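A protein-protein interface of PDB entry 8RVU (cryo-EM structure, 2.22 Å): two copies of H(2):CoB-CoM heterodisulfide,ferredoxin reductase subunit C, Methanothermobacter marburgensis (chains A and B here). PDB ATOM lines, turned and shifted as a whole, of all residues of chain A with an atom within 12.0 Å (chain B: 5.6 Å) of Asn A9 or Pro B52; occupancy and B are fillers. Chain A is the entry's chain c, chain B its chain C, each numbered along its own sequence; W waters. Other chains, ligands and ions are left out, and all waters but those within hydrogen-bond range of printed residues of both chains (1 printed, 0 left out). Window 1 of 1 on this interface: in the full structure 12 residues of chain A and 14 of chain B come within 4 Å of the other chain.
No position is printed for both chains.
N of Gln A5 lies within hydrogen-bond range of O of Arg B50, at 2.8 Å. OD1 of Asn A9 lies close to O of Thr B51, 3.2 Å away. The side-chain amide oxygen (OD1) of Asn A9 sits at hydrogen-bond distance from the guanidinium group (NH2) of Arg B54, 3.0 Å away. O of Asn A9 sits close to O of Gly B48 (3.5 Å). OD1 of Asn A9 sits close to N of Pro B52 (3.5 Å).
The side-chain hydroxyl (OG1) of Thr A2 sits at hydrogen-bond distance from the backbone NH (N) of Leu A4, 3.1 Å away. OE1 of Gln A5 lies close to N of Glu A7, 3.5 Å away. The side-chain amide oxygen (OE1) of Gln A5 lies within hydrogen-bond range of the backbone NH (N) of Glu A8 (3.0 Å). The backbone carbonyl oxygen (O) of Gln A5 is in hydrogen-bond range of the side-chain amide nitrogen (ND2) of Asn A9 (3.1 Å). The backbone carbonyl oxygen (O) of Ser B47 lies within hydrogen-bond range of the side-chain hydroxyl (OG1) of Thr B51, 2.8 Å away. The backbone carbonyl oxygen (O) of Pro B52 lies close to the guanidinium group (NH1) of Arg B54, 3.5 Å away.
Leu A3 touches Arg B50. CA of Thr B51 touches O of Leu A3, 3.8 Å away. Leu A3 touches Pro B52 (O to CD, 3.6 Å). Thr B75 touches Leu A3 (N to CD1, 3.9 Å). CA of Leu A4 touches O of Arg B50, at 3.5 Å. Arg B49 touches Asn A9. Asn A9 touches Arg B50. Ile A10 touches Arg B49 (CD1 to CD, 3.8 Å).
Of the printed residues of chain B, Gln A5 touches Arg B50 (2.8 Å). Printed residues of chain B within 4 Å of Ile A10: Arg B49 (3.8 Å). Gly B48 touches one residue of chain A. Of the printed residues of chain A, Arg B49 touches Asn A9 and Ile A10. Of chain A, only Leu A3 (3.8 Å) and Asn A9 (3.2 Å) come within 4 Å of Thr B51. Of chain A, only Leu A3 (3.6 Å) and Asn A9 (3.5 Å) come within 4 Å of Pro B52. Of chain A, only Leu A3 (3.9 Å) comes within 4 Å of Thr B75. The nearest residue of chain A that does not touch Pro B52 is Leu A4 (5.7 Å).
Of the 9 printed residues of chain B, 7 touch a printed residue of chain A. Among the printed residues, no Asp or Glu carboxylate lies within 4 Å of a Lys or Arg side-chain nitrogen of the other chain.
Water W1 lies within hydrogen-bond range of the backbone carbonyl oxygen of Asn A9 (2.5 Å), the backbone carbonyl oxygen of Gly B48 (2.9 Å) and the guanidinium group of Arg B54 (3.4 Å).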
ATOM      1  N   THR A   2      15.074 -11.554   4.506  1.00  0.00           N
ATOM      2  CA  THR A   2      16.250 -11.938   3.734  1.00  0.00           C
ATOM      3  C   THR A   2      15.949 -13.133   2.836  1.00  0.00           C
ATOM      4  O   THR A   2      15.189 -14.026   3.209  1.00  0.00           O
ATOM      5  CB  THR A   2      17.438 -12.291   4.648  1.00  0.00           C
ATOM      6  OG1 THR A   2      18.558 -12.690   3.850  1.00  0.00           O
ATOM      7  CG2 THR A   2      17.072 -13.423   5.601  1.00  0.00           C
ATOM      8  N   LEU A   3      16.552 -13.141   1.650  1.00  0.00           N
ATOM      9  CA  LEU A   3      16.440 -14.268   0.736  1.00  0.00           C
ATOM     10  C   LEU A   3      17.461 -15.360   1.015  1.00  0.00           C
ATOM     11  O   LEU A   3      17.435 -16.397   0.344  1.00  0.00           O
ATOM     12  CB  LEU A   3      16.598 -13.793  -0.712  1.00  0.00           C
ATOM     13  CG  LEU A   3      15.409 -13.052  -1.324  1.00  0.00           C
ATOM     14  CD1 LEU A   3      15.790 -12.486  -2.679  1.00  0.00           C
ATOM     15  CD2 LEU A   3      14.200 -13.964  -1.444  1.00  0.00           C
ATOM     16  N   LEU A   4      18.353 -15.158   1.982  1.00  0.00           N
ATOM     17  CA  LEU A   4      19.391 -16.142   2.259  1.00  0.00           C
ATOM     18  C   LEU A   4      18.778 -17.438   2.773  1.00  0.00           C
ATOM     19  O   LEU A   4      17.948 -17.433   3.685  1.00  0.00           O
ATOM     20  CB  LEU A   4      20.383 -15.584   3.281  1.00  0.00           C
ATOM     21  CG  LEU A   4      21.478 -16.542   3.758  1.00  0.00           C
ATOM     22  CD1 LEU A   4      22.419 -16.892   2.618  1.00  0.00           C
ATOM     23  CD2 LEU A   4      22.248 -15.938   4.918  1.00  0.00           C
ATOM     24  N   GLN A   5      19.200 -18.553   2.180  1.00  0.00           N
ATOM     25  CA  GLN A   5      18.811 -19.876   2.661  1.00  0.00           C
ATOM     26  C   GLN A   5      19.904 -20.853   2.252  1.00  0.00           C
ATOM     27  O   GLN A   5      20.016 -21.195   1.070  1.00  0.00           O
ATOM     28  CB  GLN A   5      17.436 -20.270   2.141  1.00  0.00           C
ATOM     29  CG  GLN A   5      16.457 -20.668   3.234  1.00  0.00           C
ATOM     30  CD  GLN A   5      16.822 -21.981   3.900  1.00  0.00           C
ATOM     31  OE1 GLN A   5      17.311 -22.904   3.251  1.00  0.00           O
ATOM     32  NE2 GLN A   5      16.582 -22.069   5.202  1.00  0.00           N
ATOM     33  N   ARG A   6      20.699 -21.298   3.222  1.00  0.00           N
ATOM     34  CA  ARG A   6      21.923 -22.032   2.930  1.00  0.00           C
ATOM     35  C   ARG A   6      21.692 -23.485   2.520  1.00  0.00           C
ATOM     36  O   ARG A   6      22.555 -24.076   1.862  1.00  0.00           O
ATOM     37  CB  ARG A   6      22.857 -21.948   4.141  1.00  0.00           C
ATOM     38  CG  ARG A   6      23.428 -20.556   4.382  1.00  0.00           C
ATOM     39  CD  ARG A   6      24.580 -20.574   5.379  1.00  0.00           C
ATOM     40  NE  ARG A   6      24.158 -21.025   6.701  1.00  0.00           N
ATOM     41  CZ  ARG A   6      23.643 -20.245   7.643  1.00  0.00           C
ATOM     42  NH1 ARG A   6      23.433 -18.954   7.440  1.00  0.00           N
ATOM     43  NH2 ARG A   6      23.325 -20.776   8.822  1.00  0.00           N
ATOM     44  N   GLU A   7      20.547 -24.066   2.876  1.00  0.00           N
ATOM     45  CA  GLU A   7      20.279 -25.474   2.611  1.00  0.00           C
ATOM     46  C   GLU A   7      19.288 -25.775   1.501  1.00  0.00           C
ATOM     47  O   GLU A   7      19.415 -26.809   0.843  1.00  0.00           O
ATOM     48  CB  GLU A   7      19.752 -26.087   3.915  1.00  0.00           C
ATOM     49  CG  GLU A   7      20.778 -26.146   5.033  1.00  0.00           C
ATOM     50  CD  GLU A   7      20.203 -26.691   6.328  1.00  0.00           C
ATOM     51  OE1 GLU A   7      18.968 -26.844   6.412  1.00  0.00           O
ATOM     52  OE2 GLU A   7      20.986 -26.957   7.263  1.00  0.00           O
ATOM     53  N   GLU A   8      18.308 -24.903   1.276  1.00  0.00           N
ATOM     54  CA  GLU A   8      17.241 -25.178   0.325  1.00  0.00           C
ATOM     55  C   GLU A   8      17.669 -24.988  -1.126  1.00  0.00           C
ATOM     56  O   GLU A   8      16.999 -25.510  -2.023  1.00  0.00           O
ATOM     57  CB  GLU A   8      16.037 -24.281   0.648  1.00  0.00           C
ATOM     58  CG  GLU A   8      15.224 -23.796  -0.546  1.00  0.00           C
ATOM     59  CD  GLU A   8      13.814 -23.399  -0.156  1.00  0.00           C
ATOM     60  OE1 GLU A   8      12.861 -23.844  -0.831  1.00  0.00           O
ATOM     61  OE2 GLU A   8      13.659 -22.647   0.828  1.00  0.00           O
ATOM     62  N   ASN A   9      18.776 -24.289  -1.380  1.00  0.00           N
ATOM     63  CA  ASN A   9      19.139 -23.879  -2.734  1.00  0.00           C
ATOM     64  C   ASN A   9      20.354 -24.627  -3.273  1.00  0.00           C
ATOM     65  O   ASN A   9      20.986 -24.162  -4.226  1.00  0.00           O
ATOM     66  CB  ASN A   9      19.384 -22.369  -2.773  1.00  0.00           C
ATOM     67  CG  ASN A   9      18.130 -21.572  -2.475  1.00  0.00           C
ATOM     68  OD1 ASN A   9      17.172 -21.593  -3.247  1.00  0.00           O
ATOM     69  ND2 ASN A   9      18.127 -20.867  -1.351  1.00  0.00           N
ATOM     70  N   ILE A  10      20.695 -25.775  -2.695  1.00  0.00           N
ATOM     71  CA  ILE A  10      21.802 -26.583  -3.195  1.00  0.00           C
ATOM     72  C   ILE A  10      21.569 -28.028  -2.785  1.00  0.00           C
ATOM     73  O   ILE A  10      21.058 -28.303  -1.695  1.00  0.00           O
ATOM     74  CB  ILE A  10      23.160 -26.064  -2.678  1.00  0.00           C
ATOM     75  CG1 ILE A  10      24.304 -26.661  -3.498  1.00  0.00           C
ATOM     76  CG2 ILE A  10      23.336 -26.397  -1.205  1.00  0.00           C
ATOM     77  CD1 ILE A  10      25.599 -25.903  -3.362  1.00  0.00           C
ATOM     78  N   ILE A  11      21.950 -28.954  -3.661  1.00  0.00           N
ATOM     79  CA  ILE A  11      21.794 -30.385  -3.428  1.00  0.00           C
ATOM     80  C   ILE A  11      23.179 -30.992  -3.262  1.00  0.00           C
ATOM     81  O   ILE A  11      24.039 -30.849  -4.141  1.00  0.00           O
ATOM     82  CB  ILE A  11      21.032 -31.074  -4.570  1.00  0.00           C
ATOM     83  CG1 ILE A  11      19.739 -30.320  -4.890  1.00  0.00           C
ATOM     84  CG2 ILE A  11      20.725 -32.518  -4.201  1.00  0.00           C
ATOM     85  CD1 ILE A  11      18.993 -30.867  -6.091  1.00  0.00           C
ATOM     86  N   ARG A  12      23.394 -31.668  -2.138  1.00  0.00           N
ATOM     87  CA  ARG A  12      24.616 -32.413  -1.873  1.00  0.00           C
ATOM     88  C   ARG A  12      24.238 -33.845  -1.516  1.00  0.00           C
ATOM     89  O   ARG A  12      23.067 -34.232  -1.568  1.00  0.00           O
ATOM     90  CB  ARG A  12      25.432 -31.756  -0.753  1.00  0.00           C
ATOM     91  CG  ARG A  12      25.865 -30.333  -1.064  1.00  0.00           C
ATOM     92  CD  ARG A  12      27.160 -29.975  -0.358  1.00  0.00           C
ATOM     93  NE  ARG A  12      27.597 -28.619  -0.670  1.00  0.00           N
ATOM     94  CZ  ARG A  12      27.114 -27.524  -0.098  1.00  0.00           C
ATOM     95  NH1 ARG A  12      26.176 -27.586   0.832  1.00  0.00           N
ATOM     96  NH2 ARG A  12      27.587 -26.338  -0.468  1.00  0.00           N
ATOM     97  N   LYS A  13      25.241 -34.646  -1.148  1.00  0.00           N
ATOM     98  CA  LYS A  13      24.969 -36.028  -0.772  1.00  0.00           C
ATOM     99  C   LYS A  13      24.153 -36.123   0.510  1.00  0.00           C
ATOM    100  O   LYS A  13      23.557 -37.171   0.777  1.00  0.00           O
ATOM    101  CB  LYS A  13      26.278 -36.804  -0.618  1.00  0.00           C
ATOM    102  CG  LYS A  13      27.211 -36.264   0.451  1.00  0.00           C
ATOM    103  CD  LYS A  13      28.457 -37.128   0.573  1.00  0.00           C
ATOM    104  CE  LYS A  13      29.599 -36.381   1.244  1.00  0.00           C
ATOM    105  NZ  LYS A  13      29.530 -36.471   2.728  1.00  0.00           N
ATOM    106  N   GLY A  14      24.113 -35.054   1.311  1.00  0.00           N
ATOM    107  CA  GLY A  14      23.307 -35.062   2.517  1.00  0.00           C
ATOM    108  C   GLY A  14      21.815 -35.043   2.259  1.00  0.00           C
ATOM    109  O   GLY A  14      21.044 -35.488   3.114  1.00  0.00           O
ATOM    110  N   ASN A  15      21.393 -34.535   1.103  1.00  0.00           N
ATOM    111  CA  ASN A  15      19.986 -34.486   0.734  1.00  0.00           C
ATOM    112  C   ASN A  15      19.513 -35.752   0.034  1.00  0.00           C
ATOM    113  O   ASN A  15      18.326 -35.856  -0.291  1.00  0.00           O
ATOM    114  CB  ASN A  15      19.723 -33.285  -0.182  1.00  0.00           C
ATOM    115  CG  ASN A  15      20.304 -31.996   0.361  1.00  0.00           C
ATOM    116  OD1 ASN A  15      21.363 -31.549  -0.074  1.00  0.00           O
ATOM    117  ND2 ASN A  15      19.605 -31.388   1.311  1.00  0.00           N
ATOM    118  N   LYS A  61      13.130 -36.446  -8.792  1.00  0.00           N
ATOM    119  CA  LYS A  61      13.575 -36.519  -7.405  1.00  0.00           C
ATOM    120  C   LYS A  61      13.603 -37.959  -6.912  1.00  0.00           C
ATOM    121  O   LYS A  61      14.497 -38.345  -6.150  1.00  0.00           O
ATOM    122  CB  LYS A  61      12.672 -35.665  -6.515  1.00  0.00           C
ATOM    123  CG  LYS A  61      12.802 -34.171  -6.749  1.00  0.00           C
ATOM    124  CD  LYS A  61      11.888 -33.382  -5.830  1.00  0.00           C
ATOM    125  CE  LYS A  61      11.488 -32.055  -6.450  1.00  0.00           C
ATOM    126  NZ  LYS A  61      11.127 -31.040  -5.422  1.00  0.00           N
ATOM    127  N   LEU A  66      15.928 -37.897  -3.440  1.00  0.00           N
ATOM    128  CA  LEU A  66      15.609 -36.814  -2.509  1.00  0.00           C
ATOM    129  C   LEU A  66      14.354 -37.189  -1.717  1.00  0.00           C
ATOM    130  O   LEU A  66      13.246 -36.709  -1.962  1.00  0.00           O
ATOM    131  CB  LEU A  66      15.435 -35.504  -3.266  1.00  0.00           C
ATOM    132  CG  LEU A  66      16.633 -35.084  -4.123  1.00  0.00           C
ATOM    133  CD1 LEU A  66      16.251 -33.974  -5.089  1.00  0.00           C
ATOM    134  CD2 LEU A  66      17.801 -34.654  -3.253  1.00  0.00           C
ATOM    135  N   GLU A  69      12.533 -34.300   0.387  1.00  0.00           N
ATOM    136  CA  GLU A  69      11.849 -33.339  -0.470  1.00  0.00           C
ATOM    137  C   GLU A  69      10.553 -33.916  -1.022  1.00  0.00           C
ATOM    138  O   GLU A  69       9.614 -33.169  -1.320  1.00  0.00           O
ATOM    139  CB  GLU A  69      12.772 -32.910  -1.609  1.00  0.00           C
ATOM    140  CG  GLU A  69      12.606 -31.462  -2.019  1.00  0.00           C
ATOM    141  CD  GLU A  69      13.771 -30.959  -2.844  1.00  0.00           C
ATOM    142  OE1 GLU A  69      13.726 -29.793  -3.286  1.00  0.00           O
ATOM    143  OE2 GLU A  69      14.731 -31.729  -3.050  1.00  0.00           O
ATOM    144  N   SER B  47      25.627 -16.593  -5.786  1.00  0.00           N
ATOM    145  CA  SER B  47      24.385 -16.243  -5.109  1.00  0.00           C
ATOM    146  C   SER B  47      23.309 -17.298  -5.324  1.00  0.00           C
ATOM    147  O   SER B  47      22.444 -17.480  -4.460  1.00  0.00           O
ATOM    148  CB  SER B  47      23.886 -14.879  -5.587  1.00  0.00           C
ATOM    149  OG  SER B  47      23.613 -14.888  -6.975  1.00  0.00           O
ATOM    150  N   GLY B  48      23.345 -18.002  -6.456  1.00  0.00           N
ATOM    151  CA  GLY B  48      22.389 -19.065  -6.700  1.00  0.00           C
ATOM    152  C   GLY B  48      22.542 -20.246  -5.765  1.00  0.00           C
ATOM    153  O   GLY B  48      21.617 -21.056  -5.646  1.00  0.00           O
ATOM    154  N   ARG B  49      23.691 -20.365  -5.099  1.00  0.00           N
ATOM    155  CA  ARG B  49      23.911 -21.457  -4.161  1.00  0.00           C
ATOM    156  C   ARG B  49      23.264 -21.208  -2.806  1.00  0.00           C
ATOM    157  O   ARG B  49      23.101 -22.155  -2.031  1.00  0.00           O
ATOM    158  CB  ARG B  49      25.411 -21.682  -3.959  1.00  0.00           C
ATOM    159  CG  ARG B  49      26.168 -22.039  -5.223  1.00  0.00           C
ATOM    160  CD  ARG B  49      27.394 -22.882  -4.914  1.00  0.00           C
ATOM    161  NE  ARG B  49      28.453 -22.109  -4.275  1.00  0.00           N
ATOM    162  CZ  ARG B  49      29.281 -21.292  -4.912  1.00  0.00           C
ATOM    163  NH1 ARG B  49      29.205 -21.109  -6.219  1.00  0.00           N
ATOM    164  NH2 ARG B  49      30.213 -20.645  -4.218  1.00  0.00           N
ATOM    165  N   ARG B  50      22.897 -19.962  -2.502  1.00  0.00           N
ATOM    166  CA  ARG B  50      22.371 -19.609  -1.193  1.00  0.00           C
ATOM    167  C   ARG B  50      21.091 -18.789  -1.257  1.00  0.00           C
ATOM    168  O   ARG B  50      20.582 -18.386  -0.206  1.00  0.00           O
ATOM    169  CB  ARG B  50      23.430 -18.835  -0.390  1.00  0.00           C
ATOM    170  CG  ARG B  50      23.789 -17.479  -0.974  1.00  0.00           C
ATOM    171  CD  ARG B  50      25.219 -17.093  -0.637  1.00  0.00           C
ATOM    172  NE  ARG B  50      26.173 -17.738  -1.534  1.00  0.00           N
ATOM    173  CZ  ARG B  50      27.348 -18.235  -1.171  1.00  0.00           C
ATOM    174  NH1 ARG B  50      27.777 -18.168   0.079  1.00  0.00           N
ATOM    175  NH2 ARG B  50      28.117 -18.812  -2.088  1.00  0.00           N
ATOM    176  N   THR B  51      20.562 -18.524  -2.447  1.00  0.00           N
ATOM    177  CA  THR B  51      19.306 -17.804  -2.601  1.00  0.00           C
ATOM    178  C   THR B  51      18.494 -18.463  -3.709  1.00  0.00           C
ATOM    179  O   THR B  51      19.033 -19.281  -4.465  1.00  0.00           O
ATOM    180  CB  THR B  51      19.546 -16.326  -2.929  1.00  0.00           C
ATOM    181  OG1 THR B  51      19.953 -16.193  -4.296  1.00  0.00           O
ATOM    182  CG2 THR B  51      20.614 -15.733  -2.023  1.00  0.00           C
ATOM    183  N   PRO B  52      17.205 -18.147  -3.840  1.00  0.00           N
ATOM    184  CA  PRO B  52      16.413 -18.680  -4.955  1.00  0.00           C
ATOM    185  C   PRO B  52      16.741 -18.069  -6.308  1.00  0.00           C
ATOM    186  O   PRO B  52      16.034 -18.351  -7.279  1.00  0.00           O
ATOM    187  CB  PRO B  52      14.966 -18.340  -4.549  1.00  0.00           C
ATOM    188  CG  PRO B  52      15.028 -17.857  -3.134  1.00  0.00           C
ATOM    189  CD  PRO B  52      16.395 -17.318  -2.936  1.00  0.00           C
ATOM    190  N   TYR B  53      17.781 -17.246  -6.396  1.00  0.00           N
ATOM    191  CA  TYR B  53      18.144 -16.611  -7.653  1.00  0.00           C
ATOM    192  C   TYR B  53      18.676 -17.648  -8.636  1.00  0.00           C
ATOM    193  O   TYR B  53      19.591 -18.412  -8.315  1.00  0.00           O
ATOM    194  CB  TYR B  53      19.187 -15.525  -7.396  1.00  0.00           C
ATOM    195  CG  TYR B  53      19.755 -14.884  -8.639  1.00  0.00           C
ATOM    196  CD1 TYR B  53      18.934 -14.231  -9.547  1.00  0.00           C
ATOM    197  CD2 TYR B  53      21.117 -14.922  -8.898  1.00  0.00           C
ATOM    198  CE1 TYR B  53      19.453 -13.640 -10.681  1.00  0.00           C
ATOM    199  CE2 TYR B  53      21.647 -14.334 -10.028  1.00  0.00           C
ATOM    200  CZ  TYR B  53      20.810 -13.694 -10.916  1.00  0.00           C
ATOM    201  OH  TYR B  53      21.335 -13.108 -12.044  1.00  0.00           O
ATOM    202  N   ARG B  54      18.094 -17.673  -9.833  1.00  0.00           N
ATOM    203  CA  ARG B  54      18.502 -18.581 -10.905  1.00  0.00           C
ATOM    204  C   ARG B  54      18.703 -17.732 -12.157  1.00  0.00           C
ATOM    205  O   ARG B  54      17.732 -17.332 -12.804  1.00  0.00           O
ATOM    206  CB  ARG B  54      17.462 -19.674 -11.138  1.00  0.00           C
ATOM    207  CG  ARG B  54      17.080 -20.468  -9.897  1.00  0.00           C
ATOM    208  CD  ARG B  54      18.145 -21.485  -9.519  1.00  0.00           C
ATOM    209  NE  ARG B  54      17.779 -22.232  -8.320  1.00  0.00           N
ATOM    210  CZ  ARG B  54      17.992 -21.820  -7.077  1.00  0.00           C
ATOM    211  NH1 ARG B  54      18.586 -20.666  -6.822  1.00  0.00           N
ATOM    212  NH2 ARG B  54      17.598 -22.586  -6.064  1.00  0.00           N
ATOM    213  N   THR B  75      14.628 -11.745  -6.318  1.00  0.00           N
ATOM    214  CA  THR B  75      15.883 -12.440  -6.581  1.00  0.00           C
ATOM    215  C   THR B  75      16.694 -11.758  -7.672  1.00  0.00           C
ATOM    216  O   THR B  75      17.909 -11.977  -7.755  1.00  0.00           O
ATOM    217  CB  THR B  75      15.618 -13.895  -6.973  1.00  0.00           C
ATOM    218  OG1 THR B  75      14.823 -13.938  -8.164  1.00  0.00           O
ATOM    219  CG2 THR B  75      14.896 -14.629  -5.854  1.00  0.00           C
HETATM  220  O   HOH W   1      20.776 -23.623  -6.672  1.00  0.00           O
